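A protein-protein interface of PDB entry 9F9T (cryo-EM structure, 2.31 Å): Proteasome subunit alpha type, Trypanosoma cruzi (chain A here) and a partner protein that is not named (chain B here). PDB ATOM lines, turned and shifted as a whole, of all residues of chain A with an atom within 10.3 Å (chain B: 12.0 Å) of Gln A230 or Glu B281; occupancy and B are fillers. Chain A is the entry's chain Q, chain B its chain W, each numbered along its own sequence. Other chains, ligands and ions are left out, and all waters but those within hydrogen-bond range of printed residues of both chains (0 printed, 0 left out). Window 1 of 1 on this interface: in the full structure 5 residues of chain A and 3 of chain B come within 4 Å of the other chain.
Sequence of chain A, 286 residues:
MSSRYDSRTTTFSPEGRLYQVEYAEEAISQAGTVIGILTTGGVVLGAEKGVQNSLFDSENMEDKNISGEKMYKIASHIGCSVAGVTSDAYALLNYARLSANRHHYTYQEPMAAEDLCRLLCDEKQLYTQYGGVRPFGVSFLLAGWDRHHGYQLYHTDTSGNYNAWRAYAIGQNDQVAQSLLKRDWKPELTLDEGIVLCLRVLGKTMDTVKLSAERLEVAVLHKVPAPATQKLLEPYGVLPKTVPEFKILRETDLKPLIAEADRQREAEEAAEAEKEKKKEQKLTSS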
ATOM      1  N   ALA A 226       9.078  -7.777 -24.209  1.00  0.00           N
ATOM      2  CA  ALA A 226       9.054  -7.983 -22.772  1.00  0.00           C
ATOM      3  C   ALA A 226       7.963  -8.987 -22.419  1.00  0.00           C
ATOM      4  O   ALA A 226       6.868  -8.922 -22.985  1.00  0.00           O
ATOM      5  CB  ALA A 226       8.813  -6.661 -22.079  1.00  0.00           C
ATOM      6  N   PRO A 227       8.212  -9.891 -21.439  1.00  0.00           N
ATOM      7  CA  PRO A 227       7.213 -10.878 -21.029  1.00  0.00           C
ATOM      8  C   PRO A 227       6.041 -10.246 -20.267  1.00  0.00           C
ATOM      9  O   PRO A 227       5.916  -9.021 -20.198  1.00  0.00           O
ATOM     10  CB  PRO A 227       8.059 -11.842 -20.171  1.00  0.00           C
ATOM     11  CG  PRO A 227       9.088 -10.950 -19.528  1.00  0.00           C
ATOM     12  CD  PRO A 227       9.440  -9.974 -20.629  1.00  0.00           C
ATOM     13  N   ALA A 228       5.181 -11.118 -19.718  1.00  0.00           N
ATOM     14  CA  ALA A 228       4.058 -10.760 -18.861  1.00  0.00           C
ATOM     15  C   ALA A 228       4.327  -9.487 -18.058  1.00  0.00           C
ATOM     16  O   ALA A 228       5.426  -9.283 -17.542  1.00  0.00           O
ATOM     17  CB  ALA A 228       3.763 -11.913 -17.924  1.00  0.00           C
ATOM     18  N   THR A 229       3.291  -8.652 -17.939  1.00  0.00           N
ATOM     19  CA  THR A 229       3.263  -7.556 -16.984  1.00  0.00           C
ATOM     20  C   THR A 229       2.341  -7.957 -15.830  1.00  0.00           C
ATOM     21  O   THR A 229       1.122  -7.976 -16.005  1.00  0.00           O
ATOM     22  CB  THR A 229       2.847  -6.249 -17.678  1.00  0.00           C
ATOM     23  OG1 THR A 229       1.939  -6.559 -18.738  1.00  0.00           O
ATOM     24  CG2 THR A 229       4.021  -5.483 -18.250  1.00  0.00           C
ATOM     25  N   GLN A 230       2.939  -8.292 -14.671  1.00  0.00           N
ATOM     26  CA  GLN A 230       2.203  -8.749 -13.496  1.00  0.00           C
ATOM     27  C   GLN A 230       1.703  -7.561 -12.685  1.00  0.00           C
ATOM     28  O   GLN A 230       2.203  -7.319 -11.606  1.00  0.00           O
ATOM     29  CB  GLN A 230       3.079  -9.570 -12.541  1.00  0.00           C
ATOM     30  CG  GLN A 230       3.593 -10.890 -13.097  1.00  0.00           C
ATOM     31  CD  GLN A 230       4.699 -11.459 -12.232  1.00  0.00           C
ATOM     32  OE1 GLN A 230       5.643 -10.769 -11.847  1.00  0.00           O
ATOM     33  NE2 GLN A 230       4.602 -12.740 -11.919  1.00  0.00           N
ATOM     34  N   LYS A 231       0.703  -6.845 -13.189  1.00  0.00           N
ATOM     35  CA  LYS A 231       0.247  -5.619 -12.556  1.00  0.00           C
ATOM     36  C   LYS A 231      -0.522  -5.890 -11.261  1.00  0.00           C
ATOM     37  O   LYS A 231      -0.861  -4.940 -10.559  1.00  0.00           O
ATOM     38  CB  LYS A 231      -0.619  -4.807 -13.534  1.00  0.00           C
ATOM     39  CG  LYS A 231       0.139  -3.785 -14.373  1.00  0.00           C
ATOM     40  CD  LYS A 231      -0.598  -3.381 -15.631  1.00  0.00           C
ATOM     41  CE  LYS A 231       0.320  -2.791 -16.682  1.00  0.00           C
ATOM     42  NZ  LYS A 231      -0.146  -3.108 -18.054  1.00  0.00           N
ATOM     43  N   LEU A 232      -0.875  -7.154 -10.978  1.00  0.00           N
ATOM     44  CA  LEU A 232      -1.631  -7.465  -9.773  1.00  0.00           C
ATOM     45  C   LEU A 232      -0.676  -7.723  -8.624  1.00  0.00           C
ATOM     46  O   LEU A 232      -0.956  -7.245  -7.531  1.00  0.00           O
ATOM     47  CB  LEU A 232      -2.555  -8.665 -10.014  1.00  0.00           C
ATOM     48  CG  LEU A 232      -3.456  -8.475 -11.228  1.00  0.00           C
ATOM     49  CD1 LEU A 232      -4.564  -9.516 -11.276  1.00  0.00           C
ATOM     50  CD2 LEU A 232      -4.030  -7.052 -11.235  1.00  0.00           C
ATOM     51  N   LEU A 233       0.426  -8.450  -8.880  1.00  0.00           N
ATOM     52  CA  LEU A 233       1.440  -8.694  -7.854  1.00  0.00           C
ATOM     53  C   LEU A 233       2.372  -7.487  -7.678  1.00  0.00           C
ATOM     54  O   LEU A 233       3.029  -7.392  -6.648  1.00  0.00           O
ATOM     55  CB  LEU A 233       2.259  -9.963  -8.151  1.00  0.00           C
ATOM     56  CG  LEU A 233       1.510 -11.303  -8.204  1.00  0.00           C
ATOM     57  CD1 LEU A 233       2.454 -12.453  -7.915  1.00  0.00           C
ATOM     58  CD2 LEU A 233       0.325 -11.366  -7.249  1.00  0.00           C
ATOM     59  N   GLU A 234       2.398  -6.537  -8.612  1.00  0.00           N
ATOM     60  CA  GLU A 234       3.258  -5.353  -8.517  1.00  0.00           C
ATOM     61  C   GLU A 234       2.547  -4.173  -9.153  1.00  0.00           C
ATOM     62  O   GLU A 234       2.733  -3.935 -10.339  1.00  0.00           O
ATOM     63  CB  GLU A 234       4.549  -5.428  -9.341  1.00  0.00           C
ATOM     64  CG  GLU A 234       5.719  -6.063  -8.636  1.00  0.00           C
ATOM     65  CD  GLU A 234       5.929  -7.526  -8.964  1.00  0.00           C
ATOM     66  OE1 GLU A 234       6.514  -7.821 -10.048  1.00  0.00           O
ATOM     67  OE2 GLU A 234       5.507  -8.365  -8.131  1.00  0.00           O
ATOM     68  N   PRO A 235       1.684  -3.432  -8.433  1.00  0.00           N
ATOM     69  CA  PRO A 235       0.923  -2.374  -9.090  1.00  0.00           C
ATOM     70  C   PRO A 235       1.749  -1.160  -9.496  1.00  0.00           C
ATOM     71  O   PRO A 235       1.283  -0.302 -10.231  1.00  0.00           O
ATOM     72  CB  PRO A 235      -0.218  -2.069  -8.097  1.00  0.00           C
ATOM     73  CG  PRO A 235      -0.149  -3.198  -7.039  1.00  0.00           C
ATOM     74  CD  PRO A 235       1.283  -3.684  -7.039  1.00  0.00           C
ATOM     75  N   TYR A 236       2.974  -1.066  -9.029  1.00  0.00           N
ATOM     76  CA  TYR A 236       3.833   0.040  -9.438  1.00  0.00           C
ATOM     77  C   TYR A 236       5.053  -0.545 -10.161  1.00  0.00           C
ATOM     78  O   TYR A 236       6.107   0.068 -10.208  1.00  0.00           O
ATOM     79  CB  TYR A 236       4.212   0.925  -8.232  1.00  0.00           C
ATOM     80  CG  TYR A 236       3.117   1.719  -7.526  1.00  0.00           C
ATOM     81  CD1 TYR A 236       2.684   2.964  -7.976  1.00  0.00           C
ATOM     82  CD2 TYR A 236       2.508   1.218  -6.389  1.00  0.00           C
ATOM     83  CE1 TYR A 236       1.705   3.697  -7.303  1.00  0.00           C
ATOM     84  CE2 TYR A 236       1.511   1.918  -5.724  1.00  0.00           C
ATOM     85  CZ  TYR A 236       1.096   3.159  -6.178  1.00  0.00           C
ATOM     86  OH  TYR A 236       0.104   3.772  -5.446  1.00  0.00           O
ATOM     87  N   GLY A 237       4.919  -1.747 -10.703  1.00  0.00           N
ATOM     88  CA  GLY A 237       5.876  -2.240 -11.681  1.00  0.00           C
ATOM     89  C   GLY A 237       5.686  -1.566 -13.046  1.00  0.00           C
ATOM     90  O   GLY A 237       4.562  -1.329 -13.487  1.00  0.00           O
ATOM     91  N   VAL A 238       6.799  -1.247 -13.709  1.00  0.00           N
ATOM     92  CA  VAL A 238       6.739  -0.770 -15.081  1.00  0.00           C
ATOM     93  C   VAL A 238       7.872  -1.446 -15.849  1.00  0.00           C
ATOM     94  O   VAL A 238       9.039  -1.340 -15.465  1.00  0.00           O
ATOM     95  CB  VAL A 238       6.794   0.772 -15.182  1.00  0.00           C
ATOM     96  CG1 VAL A 238       6.373   1.266 -16.567  1.00  0.00           C
ATOM     97  CG2 VAL A 238       5.955   1.450 -14.105  1.00  0.00           C
ATOM     98  N   LEU A 239       7.495  -2.164 -16.912  1.00  0.00           N
ATOM     99  CA  LEU A 239       8.471  -2.778 -17.793  1.00  0.00           C
ATOM    100  C   LEU A 239       8.475  -2.034 -19.124  1.00  0.00           C
ATOM    101  O   LEU A 239       7.468  -1.485 -19.572  1.00  0.00           O
ATOM    102  CB  LEU A 239       8.164  -4.269 -17.992  1.00  0.00           C
ATOM    103  CG  LEU A 239       8.590  -5.230 -16.875  1.00  0.00           C
ATOM    104  CD1 LEU A 239       8.425  -6.676 -17.338  1.00  0.00           C
ATOM    105  CD2 LEU A 239      10.027  -4.981 -16.416  1.00  0.00           C
ATOM    106  N   PRO B 276     -16.578 -12.615  -6.061  1.00  0.00           N
ATOM    107  CA  PRO B 276     -16.364 -11.512  -7.005  1.00  0.00           C
ATOM    108  C   PRO B 276     -14.919 -11.067  -7.275  1.00  0.00           C
ATOM    109  O   PRO B 276     -14.239 -10.519  -6.414  1.00  0.00           O
ATOM    110  CB  PRO B 276     -17.098 -10.326  -6.344  1.00  0.00           C
ATOM    111  CG  PRO B 276     -18.148 -10.985  -5.492  1.00  0.00           C
ATOM    112  CD  PRO B 276     -17.407 -12.171  -4.928  1.00  0.00           C
ATOM    113  N   VAL B 277     -14.491 -11.250  -8.517  1.00  0.00           N
ATOM    114  CA  VAL B 277     -13.157 -10.865  -8.945  1.00  0.00           C
ATOM    115  C   VAL B 277     -13.248  -9.519  -9.677  1.00  0.00           C
ATOM    116  O   VAL B 277     -14.135  -9.276 -10.501  1.00  0.00           O
ATOM    117  CB  VAL B 277     -12.578 -12.031  -9.767  1.00  0.00           C
ATOM    118  CG1 VAL B 277     -11.375 -11.655 -10.594  1.00  0.00           C
ATOM    119  CG2 VAL B 277     -12.273 -13.216  -8.864  1.00  0.00           C
ATOM    120  N   LEU B 278     -12.325  -8.613  -9.341  1.00  0.00           N
ATOM    121  CA  LEU B 278     -12.252  -7.325 -10.007  1.00  0.00           C
ATOM    122  C   LEU B 278     -11.456  -7.498 -11.280  1.00  0.00           C
ATOM    123  O   LEU B 278     -11.764  -6.820 -12.253  1.00  0.00           O
ATOM    124  CB  LEU B 278     -11.610  -6.259  -9.101  1.00  0.00           C
ATOM    125  CG  LEU B 278     -12.432  -5.848  -7.874  1.00  0.00           C
ATOM    126  CD1 LEU B 278     -11.629  -4.943  -6.945  1.00  0.00           C
ATOM    127  CD2 LEU B 278     -13.752  -5.186  -8.280  1.00  0.00           C
ATOM    128  N   ARG B 279     -10.422  -8.344 -11.244  1.00  0.00           N
ATOM    129  CA  ARG B 279      -9.400  -8.343 -12.280  1.00  0.00           C
ATOM    130  C   ARG B 279      -8.655  -9.675 -12.325  1.00  0.00           C
ATOM    131  O   ARG B 279      -8.375 -10.279 -11.301  1.00  0.00           O
ATOM    132  CB  ARG B 279      -8.429  -7.186 -12.055  1.00  0.00           C
ATOM    133  CG  ARG B 279      -8.752  -5.929 -12.850  1.00  0.00           C
ATOM    134  CD  ARG B 279      -7.796  -4.779 -12.535  1.00  0.00           C
ATOM    135  NE  ARG B 279      -6.515  -4.907 -13.234  1.00  0.00           N
ATOM    136  CZ  ARG B 279      -5.386  -4.286 -12.884  1.00  0.00           C
ATOM    137  NH1 ARG B 279      -4.339  -4.312 -13.693  1.00  0.00           N
ATOM    138  NH2 ARG B 279      -5.317  -3.605 -11.750  1.00  0.00           N
ATOM    139  N   GLU B 280      -8.286 -10.087 -13.538  1.00  0.00           N
ATOM    140  CA  GLU B 280      -7.713 -11.402 -13.790  1.00  0.00           C
ATOM    141  C   GLU B 280      -6.565 -11.242 -14.778  1.00  0.00           C
ATOM    142  O   GLU B 280      -6.680 -10.463 -15.716  1.00  0.00           O
ATOM    143  CB  GLU B 280      -8.815 -12.335 -14.317  1.00  0.00           C
ATOM    144  CG  GLU B 280      -8.358 -13.761 -14.626  1.00  0.00           C
ATOM    145  CD  GLU B 280      -9.457 -14.821 -14.765  1.00  0.00           C
ATOM    146  OE1 GLU B 280     -10.323 -14.937 -13.851  1.00  0.00           O
ATOM    147  OE2 GLU B 280      -9.431 -15.569 -15.771  1.00  0.00           O
ATOM    148  N   GLU B 281      -5.482 -11.987 -14.589  1.00  0.00           N
ATOM    149  CA  GLU B 281      -4.490 -12.158 -15.640  1.00  0.00           C
ATOM    150  C   GLU B 281      -4.085 -13.625 -15.748  1.00  0.00           C
ATOM    151  O   GLU B 281      -4.132 -14.349 -14.765  1.00  0.00           O
ATOM    152  CB  GLU B 281      -3.277 -11.258 -15.392  1.00  0.00           C
ATOM    153  CG  GLU B 281      -3.575  -9.768 -15.578  1.00  0.00           C
ATOM    154  CD  GLU B 281      -2.443  -8.801 -15.234  1.00  0.00           C
ATOM    155  OE1 GLU B 281      -1.377  -9.264 -14.739  1.00  0.00           O
ATOM    156  OE2 GLU B 281      -2.627  -7.575 -15.463  1.00  0.00           O
ATOM    157  N   ILE B 282      -3.645 -14.035 -16.946  1.00  0.00           N
ATOM    158  CA  ILE B 282      -3.264 -15.415 -17.238  1.00  0.00           C
ATOM    159  C   ILE B 282      -1.867 -15.432 -17.840  1.00  0.00           C
ATOM    160  O   ILE B 282      -1.388 -14.429 -18.358  1.00  0.00           O
ATOM    161  CB  ILE B 282      -4.297 -16.096 -18.157  1.00  0.00           C
ATOM    162  CG1 ILE B 282      -5.725 -15.917 -17.612  1.00  0.00           C
ATOM    163  CG2 ILE B 282      -3.931 -17.556 -18.360  1.00  0.00           C
ATOM    164  CD1 ILE B 282      -6.797 -16.722 -18.323  1.00  0.00           C
ATOM    165  N   ARG B 283      -1.184 -16.563 -17.674  1.00  0.00           N
ATOM    166  CA  ARG B 283       0.201 -16.709 -18.088  1.00  0.00           C
ATOM    167  C   ARG B 283       0.380 -18.182 -18.437  1.00  0.00           C
ATOM    168  O   ARG B 283       0.192 -19.030 -17.569  1.00  0.00           O
ATOM    169  CB  ARG B 283       1.129 -16.212 -16.962  1.00  0.00           C
ATOM    170  CG  ARG B 283       2.377 -15.452 -17.411  1.00  0.00           C
ATOM    171  CD  ARG B 283       3.381 -15.130 -16.297  1.00  0.00           C
ATOM    172  NE  ARG B 283       4.564 -16.005 -16.204  1.00  0.00           N
ATOM    173  CZ  ARG B 283       5.482 -15.973 -15.224  1.00  0.00           C
ATOM    174  NH1 ARG B 283       6.510 -16.806 -15.243  1.00  0.00           N
ATOM    175  NH2 ARG B 283       5.372 -15.124 -14.211  1.00  0.00           N
ATOM    176  N   ARG B 284       0.702 -18.481 -19.706  1.00  0.00           N
ATOM    177  CA  ARG B 284       0.906 -19.850 -20.176  1.00  0.00           C
ATOM    178  C   ARG B 284       2.337 -20.320 -19.884  1.00  0.00           C
ATOM    179  O   ARG B 284       3.302 -19.615 -20.201  1.00  0.00           O
ATOM    180  CB  ARG B 284       0.642 -19.944 -21.683  1.00  0.00           C
ATOM    181  CG  ARG B 284      -0.795 -19.649 -22.085  1.00  0.00           C
ATOM    182  CD  ARG B 284      -1.733 -20.809 -21.815  1.00  0.00           C
ATOM    183  NE  ARG B 284      -3.125 -20.379 -21.803  1.00  0.00           N
ATOM    184  CZ  ARG B 284      -4.149 -21.164 -21.477  1.00  0.00           C
ATOM    185  NH1 ARG B 284      -3.961 -22.461 -21.295  1.00  0.00           N
ATOM    186  NH2 ARG B 284      -5.361 -20.650 -21.346  1.00  0.00           N
ATOM    187  N   LEU B 285       2.458 -21.525 -19.293  1.00  0.00           N
ATOM    188  CA  LEU B 285       3.749 -22.089 -18.915  1.00  0.00           C
ATOM    189  C   LEU B 285       4.135 -23.252 -19.852  1.00  0.00           C
ATOM    190  O   LEU B 285       3.821 -23.180 -21.062  1.00  0.00           O
ATOM    191  CB  LEU B 285       3.712 -22.563 -17.447  1.00  0.00           C
ATOM    192  CG  LEU B 285       3.228 -21.572 -16.378  1.00  0.00           C
ATOM    193  CD1 LEU B 285       3.759 -21.948 -14.998  1.00  0.00           C
ATOM    194  CD2 LEU B 285       3.602 -20.129 -16.686  1.00  0.00           C
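Of the 14 printed residues of chain A, 5 touch a printed residue of chain B.
The guanidinium group of Arg B283 lies close to the side-chain amide nitrogen of Gln A230, at 3.4 Å.
O of Thr A229 sits close to OE1 of Glu B281, 3.1 Å away.
Thr A229 touches one residue of chain B.
No residue of chain B comes within 4 Å of Leu A233.
No residue of chain B comes within 4 Å of Gly A237.
Printed residues of chain A within 4 Å of Arg B279: Lys A231 (3.8 Å) and Leu A232 (3.5 Å).
Glu B280 touches none of the printed residues of chain A.
Glu B281 touches three residues of chain A.
No residue of chain A comes within 4 Å of Ile B282.
Printed residues of chain A within 4 Å of Arg B283: Ala A228 and Gln A230.
The nearest residue of chain B that does not touch Gln A230 is Arg B279 (6.9 Å).
The nearest residue of chain A that does not touch Glu B281 is Leu A232 (4.1 Å).
Among the printed residues, pairs that only touch across the chains: Leu A232 with Arg B279 (3.5 Å), Lys A231 with Glu B281 (3.5 Å), Ala A228 with Arg B283 (3.6 Å), Lys A231 with Arg B279 (3.8 Å) and Gln A230 with Glu B281 (3.8 Å).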
